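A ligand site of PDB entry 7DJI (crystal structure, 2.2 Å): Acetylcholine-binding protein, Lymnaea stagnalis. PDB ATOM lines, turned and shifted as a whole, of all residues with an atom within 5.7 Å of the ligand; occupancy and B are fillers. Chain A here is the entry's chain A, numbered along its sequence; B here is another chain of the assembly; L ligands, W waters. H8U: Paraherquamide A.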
ATOM      1  N   TYR A  93     -19.392  13.272  17.371  1.00  0.00           N
ATOM      2  CA  TYR A  93     -18.187  12.447  17.084  1.00  0.00           C
ATOM      3  C   TYR A  93     -18.541  11.309  16.104  1.00  0.00           C
ATOM      4  O   TYR A  93     -17.676  10.997  15.270  1.00  0.00           O
ATOM      5  CB  TYR A  93     -17.569  11.960  18.396  1.00  0.00           C
ATOM      6  CG  TYR A  93     -16.964  13.050  19.265  1.00  0.00           C
ATOM      7  CD1 TYR A  93     -16.457  14.214  18.704  1.00  0.00           C
ATOM      8  CD2 TYR A  93     -16.857  12.893  20.641  1.00  0.00           C
ATOM      9  CE1 TYR A  93     -15.878  15.200  19.485  1.00  0.00           C
ATOM     10  CE2 TYR A  93     -16.283  13.873  21.440  1.00  0.00           C
ATOM     11  CZ  TYR A  93     -15.793  15.040  20.856  1.00  0.00           C
ATOM     12  OH  TYR A  93     -15.211  16.024  21.605  1.00  0.00           O
ATOM     13  N   ASN A  94     -19.755  10.751  16.164  1.00  0.00           N
ATOM     14  CA  ASN A  94     -20.163   9.592  15.326  1.00  0.00           C
ATOM     15  C   ASN A  94     -21.053  10.043  14.161  1.00  0.00           C
ATOM     16  O   ASN A  94     -21.725   9.186  13.567  1.00  0.00           O
ATOM     17  CB  ASN A  94     -20.820   8.478  16.156  1.00  0.00           C
ATOM     18  CG  ASN A  94     -22.041   8.941  16.930  1.00  0.00           C
ATOM     19  OD1 ASN A  94     -22.022  10.009  17.546  1.00  0.00           O
ATOM     20  ND2 ASN A  94     -23.080   8.130  16.932  1.00  0.00           N
ATOM     21  N   LYS A 143     -22.538  11.003  20.649  1.00  0.00           N
ATOM     22  CA  LYS A 143     -21.584  11.698  21.561  1.00  0.00           C
ATOM     23  C   LYS A 143     -21.267  13.079  20.982  1.00  0.00           C
ATOM     24  O   LYS A 143     -20.903  13.151  19.794  1.00  0.00           O
ATOM     25  CB  LYS A 143     -20.312  10.870  21.733  1.00  0.00           C
ATOM     26  CG  LYS A 143     -20.417   9.713  22.716  1.00  0.00           C
ATOM     27  CD  LYS A 143     -19.094   9.045  23.018  1.00  0.00           C
ATOM     28  CE  LYS A 143     -19.233   7.909  24.001  1.00  0.00           C
ATOM     29  NZ  LYS A 143     -17.950   7.188  24.205  1.00  0.00           N
ATOM     30  N   SER A 146     -16.329  19.180  22.394  1.00  0.00           N
ATOM     31  CA  SER A 146     -15.435  20.173  21.737  1.00  0.00           C
ATOM     32  C   SER A 146     -14.452  19.433  20.825  1.00  0.00           C
ATOM     33  O   SER A 146     -13.936  18.394  21.249  1.00  0.00           O
ATOM     34  CB  SER A 146     -14.686  20.987  22.768  1.00  0.00           C
ATOM     35  OG  SER A 146     -13.632  21.716  22.163  1.00  0.00           O
ATOM     36  N   TRP A 147     -14.183  19.974  19.636  1.00  0.00           N
ATOM     37  CA  TRP A 147     -13.198  19.361  18.708  1.00  0.00           C
ATOM     38  C   TRP A 147     -11.760  19.649  19.168  1.00  0.00           C
ATOM     39  O   TRP A 147     -10.897  18.756  18.994  1.00  0.00           O
ATOM     40  CB  TRP A 147     -13.420  19.818  17.267  1.00  0.00           C
ATOM     41  CG  TRP A 147     -12.640  18.967  16.314  1.00  0.00           C
ATOM     42  CD1 TRP A 147     -11.597  19.349  15.512  1.00  0.00           C
ATOM     43  CD2 TRP A 147     -12.782  17.546  16.123  1.00  0.00           C
ATOM     44  NE1 TRP A 147     -11.112  18.274  14.828  1.00  0.00           N
ATOM     45  CE2 TRP A 147     -11.814  17.156  15.171  1.00  0.00           C
ATOM     46  CE3 TRP A 147     -13.643  16.578  16.647  1.00  0.00           C
ATOM     47  CZ2 TRP A 147     -11.695  15.831  14.732  1.00  0.00           C
ATOM     48  CZ3 TRP A 147     -13.531  15.266  16.210  1.00  0.00           C
ATOM     49  CH2 TRP A 147     -12.566  14.903  15.275  1.00  0.00           C
ATOM     50  N   THR A 148     -11.501  20.819  19.756  1.00  0.00           N
ATOM     51  CA  THR A 148     -10.129  21.340  19.983  1.00  0.00           C
ATOM     52  C   THR A 148      -9.889  21.815  21.418  1.00  0.00           C
ATOM     53  O   THR A 148      -8.721  22.158  21.701  1.00  0.00           O
ATOM     54  CB  THR A 148      -9.821  22.465  18.979  1.00  0.00           C
ATOM     55  OG1 THR A 148     -10.592  23.617  19.309  1.00  0.00           O
ATOM     56  CG2 THR A 148     -10.098  22.042  17.551  1.00  0.00           C
ATOM     57  N   HIS A 149     -10.890  21.833  22.300  1.00  0.00           N
ATOM     58  CA  HIS A 149     -10.755  22.330  23.699  1.00  0.00           C
ATOM     59  C   HIS A 149     -10.892  21.178  24.698  1.00  0.00           C
ATOM     60  O   HIS A 149     -11.976  20.573  24.782  1.00  0.00           O
ATOM     61  CB  HIS A 149     -11.755  23.453  23.996  1.00  0.00           C
ATOM     62  CG  HIS A 149     -11.560  24.673  23.165  1.00  0.00           C
ATOM     63  ND1 HIS A 149     -10.554  25.594  23.410  1.00  0.00           N
ATOM     64  CD2 HIS A 149     -12.259  25.160  22.112  1.00  0.00           C
ATOM     65  CE1 HIS A 149     -10.636  26.581  22.541  1.00  0.00           C
ATOM     66  NE2 HIS A 149     -11.671  26.337  21.731  1.00  0.00           N
ATOM     67  N   TYR A 189      -7.310  10.451  26.023  1.00  0.00           N
ATOM     68  CA  TYR A 189      -6.991   9.766  24.738  1.00  0.00           C
ATOM     69  C   TYR A 189      -5.477   9.775  24.508  1.00  0.00           C
ATOM     70  O   TYR A 189      -4.777  10.622  25.105  1.00  0.00           O
ATOM     71  CB  TYR A 189      -7.731  10.437  23.571  1.00  0.00           C
ATOM     72  CG  TYR A 189      -9.230  10.400  23.678  1.00  0.00           C
ATOM     73  CD1 TYR A 189      -9.963   9.314  23.229  1.00  0.00           C
ATOM     74  CD2 TYR A 189      -9.934  11.449  24.247  1.00  0.00           C
ATOM     75  CE1 TYR A 189     -11.348   9.268  23.326  1.00  0.00           C
ATOM     76  CE2 TYR A 189     -11.317  11.437  24.343  1.00  0.00           C
ATOM     77  CZ  TYR A 189     -12.032  10.337  23.883  1.00  0.00           C
ATOM     78  OH  TYR A 189     -13.387  10.321  23.995  1.00  0.00           O
ATOM     79  N   CYS A 191      -3.687  10.766  22.030  1.00  0.00           N
ATOM     80  CA  CYS A 191      -3.168  11.990  21.351  1.00  0.00           C
ATOM     81  C   CYS A 191      -2.523  12.936  22.378  1.00  0.00           C
ATOM     82  O   CYS A 191      -1.434  13.459  22.082  1.00  0.00           O
ATOM     83  CB  CYS A 191      -4.259  12.763  20.608  1.00  0.00           C
ATOM     84  SG  CYS A 191      -5.480  13.600  21.668  1.00  0.00           S
ATOM     85  N   CYS A 192      -3.178  13.120  23.527  1.00  0.00           N
ATOM     86  CA  CYS A 192      -3.089  14.341  24.370  1.00  0.00           C
ATOM     87  C   CYS A 192      -3.038  13.989  25.848  1.00  0.00           C
ATOM     88  O   CYS A 192      -3.624  12.992  26.282  1.00  0.00           O
ATOM     89  CB  CYS A 192      -4.295  15.224  24.048  1.00  0.00           C
ATOM     90  SG  CYS A 192      -4.614  15.376  22.267  1.00  0.00           S
ATOM     91  N   TYR A 196     -10.592  15.195  27.757  1.00  0.00           N
ATOM     92  CA  TYR A 196     -11.686  15.820  26.971  1.00  0.00           C
ATOM     93  C   TYR A 196     -13.019  15.359  27.553  1.00  0.00           C
ATOM     94  O   TYR A 196     -13.086  14.240  28.110  1.00  0.00           O
ATOM     95  CB  TYR A 196     -11.553  15.492  25.484  1.00  0.00           C
ATOM     96  CG  TYR A 196     -10.502  16.339  24.796  1.00  0.00           C
ATOM     97  CD1 TYR A 196      -9.156  16.080  24.975  1.00  0.00           C
ATOM     98  CD2 TYR A 196     -10.860  17.408  23.989  1.00  0.00           C
ATOM     99  CE1 TYR A 196      -8.179  16.858  24.358  1.00  0.00           C
ATOM    100  CE2 TYR A 196      -9.902  18.193  23.370  1.00  0.00           C
ATOM    101  CZ  TYR A 196      -8.563  17.913  23.553  1.00  0.00           C
ATOM    102  OH  TYR A 196      -7.592  18.683  22.964  1.00  0.00           O
ATOM    103  N   ILE B  40     -12.162   6.163  10.839  1.00  0.00           N
ATOM    104  CA  ILE B  40     -13.341   6.167  11.755  1.00  0.00           C
ATOM    105  C   ILE B  40     -14.418   5.243  11.166  1.00  0.00           C
ATOM    106  O   ILE B  40     -15.109   4.582  11.959  1.00  0.00           O
ATOM    107  CB  ILE B  40     -13.877   7.603  11.981  1.00  0.00           C
ATOM    108  CG1 ILE B  40     -12.743   8.612  12.214  1.00  0.00           C
ATOM    109  CG2 ILE B  40     -14.877   7.611  13.115  1.00  0.00           C
ATOM    110  CD1 ILE B  40     -11.809   8.248  13.340  1.00  0.00           C
ATOM    111  N   TRP B  57      -9.854  10.870  10.110  1.00  0.00           N
ATOM    112  CA  TRP B  57      -9.113  12.075  10.562  1.00  0.00           C
ATOM    113  C   TRP B  57      -7.874  12.194   9.683  1.00  0.00           C
ATOM    114  O   TRP B  57      -7.107  11.213   9.623  1.00  0.00           O
ATOM    115  CB  TRP B  57      -8.710  12.011  12.046  1.00  0.00           C
ATOM    116  CG  TRP B  57      -9.823  11.720  12.997  1.00  0.00           C
ATOM    117  CD1 TRP B  57     -11.161  11.878  12.812  1.00  0.00           C
ATOM    118  CD2 TRP B  57      -9.661  11.247  14.347  1.00  0.00           C
ATOM    119  NE1 TRP B  57     -11.842  11.507  13.934  1.00  0.00           N
ATOM    120  CE2 TRP B  57     -10.953  11.116  14.894  1.00  0.00           C
ATOM    121  CE3 TRP B  57      -8.552  10.884  15.127  1.00  0.00           C
ATOM    122  CZ2 TRP B  57     -11.161  10.661  16.195  1.00  0.00           C
ATOM    123  CZ3 TRP B  57      -8.756  10.435  16.409  1.00  0.00           C
ATOM    124  CH2 TRP B  57     -10.049  10.325  16.930  1.00  0.00           C
ATOM    125  N   GLN B  59      -4.819  13.677  10.019  1.00  0.00           N
ATOM    126  CA  GLN B  59      -3.998  14.253  11.104  1.00  0.00           C
ATOM    127  C   GLN B  59      -2.788  14.922  10.439  1.00  0.00           C
ATOM    128  O   GLN B  59      -1.983  14.210   9.796  1.00  0.00           O
ATOM    129  CB  GLN B  59      -3.628  13.199  12.140  1.00  0.00           C
ATOM    130  CG  GLN B  59      -4.841  12.638  12.876  1.00  0.00           C
ATOM    131  CD  GLN B  59      -4.501  11.484  13.782  1.00  0.00           C
ATOM    132  OE1 GLN B  59      -3.938  10.472  13.354  1.00  0.00           O
ATOM    133  NE2 GLN B  59      -4.846  11.620  15.054  1.00  0.00           N
ATOM    134  N   ARG B 108      -5.211  23.547  16.519  1.00  0.00           N
ATOM    135  CA  ARG B 108      -4.549  23.786  17.824  1.00  0.00           C
ATOM    136  C   ARG B 108      -3.124  24.269  17.542  1.00  0.00           C
ATOM    137  O   ARG B 108      -2.411  23.568  16.788  1.00  0.00           O
ATOM    138  CB  ARG B 108      -4.593  22.515  18.671  1.00  0.00           C
ATOM    139  CG  ARG B 108      -4.288  22.725  20.150  1.00  0.00           C
ATOM    140  CD  ARG B 108      -5.338  23.551  20.870  1.00  0.00           C
ATOM    141  NE  ARG B 108      -5.015  23.667  22.284  1.00  0.00           N
ATOM    142  CZ  ARG B 108      -5.755  24.305  23.184  1.00  0.00           C
ATOM    143  NH1 ARG B 108      -6.884  24.900  22.827  1.00  0.00           N
ATOM    144  NH2 ARG B 108      -5.364  24.355  24.443  1.00  0.00           N
ATOM    145  N   LEU B 116      -1.459  21.805  14.921  1.00  0.00           N
ATOM    146  CA  LEU B 116      -2.150  20.489  14.839  1.00  0.00           C
ATOM    147  C   LEU B 116      -3.526  20.738  14.206  1.00  0.00           C
ATOM    148  O   LEU B 116      -4.379  21.347  14.873  1.00  0.00           O
ATOM    149  CB  LEU B 116      -2.277  19.867  16.236  1.00  0.00           C
ATOM    150  CG  LEU B 116      -0.959  19.571  16.961  1.00  0.00           C
ATOM    151  CD1 LEU B 116      -0.439  20.803  17.683  1.00  0.00           C
ATOM    152  CD2 LEU B 116      -1.125  18.421  17.945  1.00  0.00           C
ATOM    153  N   MET B 118      -6.509  18.634  12.520  1.00  0.00           N
ATOM    154  CA  MET B 118      -6.995  17.223  12.506  1.00  0.00           C
ATOM    155  C   MET B 118      -8.463  17.206  12.085  1.00  0.00           C
ATOM    156  O   MET B 118      -9.337  16.846  12.864  1.00  0.00           O
ATOM    157  CB  MET B 118      -6.844  16.570  13.876  1.00  0.00           C
ATOM    158  CG  MET B 118      -5.585  16.958  14.646  1.00  0.00           C
ATOM    159  SD  MET B 118      -4.037  16.348  13.919  1.00  0.00           S
ATOM    160  CE  MET B 118      -3.101  15.910  15.384  1.00  0.00           C
ATOM    161  N   TYR B 168     -10.104   3.870  16.772  1.00  0.00           N
ATOM    162  CA  TYR B 168     -11.269   4.792  16.681  1.00  0.00           C
ATOM    163  C   TYR B 168     -12.216   4.365  15.561  1.00  0.00           C
ATOM    164  O   TYR B 168     -13.091   5.169  15.177  1.00  0.00           O
ATOM    165  CB  TYR B 168     -10.752   6.213  16.450  1.00  0.00           C
ATOM    166  CG  TYR B 168      -9.881   6.729  17.570  1.00  0.00           C
ATOM    167  CD1 TYR B 168     -10.370   6.850  18.850  1.00  0.00           C
ATOM    168  CD2 TYR B 168      -8.567   7.086  17.335  1.00  0.00           C
ATOM    169  CE1 TYR B 168      -9.579   7.320  19.888  1.00  0.00           C
ATOM    170  CE2 TYR B 168      -7.761   7.567  18.358  1.00  0.00           C
ATOM    171  CZ  TYR B 168      -8.272   7.685  19.633  1.00  0.00           C
ATOM    172  OH  TYR B 168      -7.488   8.157  20.638  1.00  0.00           O
HETATM  173  OAV H8U L   1      -8.272  12.045  20.040  1.00  0.00           O
HETATM  174  CAP H8U L   1      -9.486  12.009  19.867  1.00  0.00           C
HETATM  175  NAO H8U L   1     -10.205  10.953  20.172  1.00  0.00           N
HETATM  176  CAN H8U L   1     -11.467  11.180  19.788  1.00  0.00           C
HETATM  177  CBA H8U L   1     -12.510  10.321  19.776  1.00  0.00           C
HETATM  178  OBF H8U L   1     -12.216   9.090  20.279  1.00  0.00           O
HETATM  179  CBE H8U L   1     -13.135   8.068  20.277  1.00  0.00           C
HETATM  180  CBD H8U L   1     -14.303   7.863  19.535  1.00  0.00           C
HETATM  181  CBC H8U L   1     -14.930   8.730  18.627  1.00  0.00           C
HETATM  182  CBG H8U L   1     -16.410   8.320  18.462  1.00  0.00           C
HETATM  183  CBH H8U L   1     -14.300   8.675  17.224  1.00  0.00           C
HETATM  184  OBB H8U L   1     -14.920  10.065  19.179  1.00  0.00           O
HETATM  185  CAZ H8U L   1     -13.728  10.737  19.286  1.00  0.00           C
HETATM  186  CAY H8U L   1     -13.819  12.040  18.812  1.00  0.00           C
HETATM  187  CAX H8U L   1     -12.711  12.877  18.832  1.00  0.00           C
HETATM  188  CAM H8U L   1     -11.539  12.446  19.309  1.00  0.00           C
HETATM  189  CAH H8U L   1     -10.274  13.083  19.420  1.00  0.00           C
HETATM  190  CAI H8U L   1      -9.770  13.578  18.064  1.00  0.00           C
HETATM  191  CAG H8U L   1     -10.170  14.329  20.401  1.00  0.00           C
HETATM  192  CBI H8U L   1     -10.092  13.895  21.872  1.00  0.00           C
HETATM  193  CBJ H8U L   1     -11.351  15.313  20.271  1.00  0.00           C
HETATM  194  CAC H8U L   1      -8.796  14.883  19.928  1.00  0.00           C
HETATM  195  CAB H8U L   1      -8.279  16.300  20.374  1.00  0.00           C
HETATM  196  CAA H8U L   1      -7.614  16.897  19.122  1.00  0.00           C
HETATM  197  CAR H8U L   1      -6.804  15.909  18.444  1.00  0.00           C
HETATM  198  OAU H8U L   1      -5.599  16.042  18.219  1.00  0.00           O
HETATM  199  NAS H8U L   1      -7.449  14.809  18.019  1.00  0.00           N
HETATM  200  CAT H8U L   1      -6.752  13.699  17.315  1.00  0.00           C
HETATM  201  CAD H8U L   1      -8.865  14.820  18.391  1.00  0.00           C
HETATM  202  CAE H8U L   1      -9.409  16.100  17.712  1.00  0.00           C
HETATM  203  NAF H8U L   1      -8.708  17.298  18.219  1.00  0.00           N
HETATM  204  CAJ H8U L   1      -8.089  18.184  17.220  1.00  0.00           C
HETATM  205  CAK H8U L   1      -6.928  18.862  17.936  1.00  0.00           C
HETATM  206  CAL H8U L   1      -6.977  18.287  19.352  1.00  0.00           C
HETATM  207  CAQ H8U L   1      -5.579  18.268  20.002  1.00  0.00           C
HETATM  208  OAW H8U L   1      -7.860  19.090  20.121  1.00  0.00           O
HETATM  209  O   HOH W   1      -7.220  20.466  14.837  1.00  0.00           O
HETATM  210  O   HOH W   2      -6.032  10.082  20.265  1.00  0.00           O
HETATM  211  O   HOH W   3      -2.880  15.142  18.325  1.00  0.00           O
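Water W2 lies within hydrogen-bond range of the side-chain hydroxyl (OH) of Tyr 168 of chain B, an oxygen (OAV) of the ligand and the backbone NH (N) of Cys 191.
An oxygen (OAV) of the ligand lies close to the side-chain sulfur (SG) of Cys 191 (3.6 Å). Tyr 93 touches the ligand (CG to CAY, 3.3 Å). Thr 148 touches the ligand. Tyr 189 touches the ligand (CE1 to OBF, 3.2 Å). SG of Cys 192 touches CAQ of the ligand, 3.8 Å away. Trp 57 of chain B touches the ligand. Gln 59 of chain B touches the ligand (NE2 to CAT, 3.6 Å). CG of Met 118 of chain B touches OAU of the ligand, 3.7 Å away. Tyr 168 of chain B touches the ligand (CE1 to OBF, 3.2 Å). Hydrophobic or aromatic side chains within 4 Å of the ligand: Tyr 93, Trp 147, Tyr 189, Tyr 196, Trp 57 of chain B, Met 118 of chain B and Tyr 168 of chain B. Of the 18 residues printed, 11 come within 4 Å of the ligand. The nearest printed residue that does not touch the ligand is Ser 146 (4.1 Å).
The backbone carbonyl oxygen (O) of Thr 148 sits at hydrogen-bond distance from the guanidinium group (NH1) of Arg 108 of chain B, 3.5 Å away. The side-chain sulfur (SG) of Cys 191 forms a disulfide with the side-chain sulfur (SG) of Cys 192. The backbone NH (N) of Tyr 93 lies within hydrogen-bond range of the backbone carbonyl oxygen (O) of Lys 143, at 2.9 Å. O of Ser 146 is in hydrogen-bond range of OH of Tyr 93, 2.7 Å away. The side-chain hydroxyl (OG) of Ser 146 lies within hydrogen-bond range of the backbone NH (N) of Thr 148 (3.3 Å). O of Met 118 of chain B sits at hydrogen-bond distance from NE1 of Trp 147 (3.0 Å).
O of Trp 147 lies within hydrogen-bond range of OAW of the ligand (3.3 Å). The side-chain hydroxyl (OH) of Tyr 196 sits at hydrogen-bond distance from an oxygen (OAW) of the ligand (2.9 Å).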
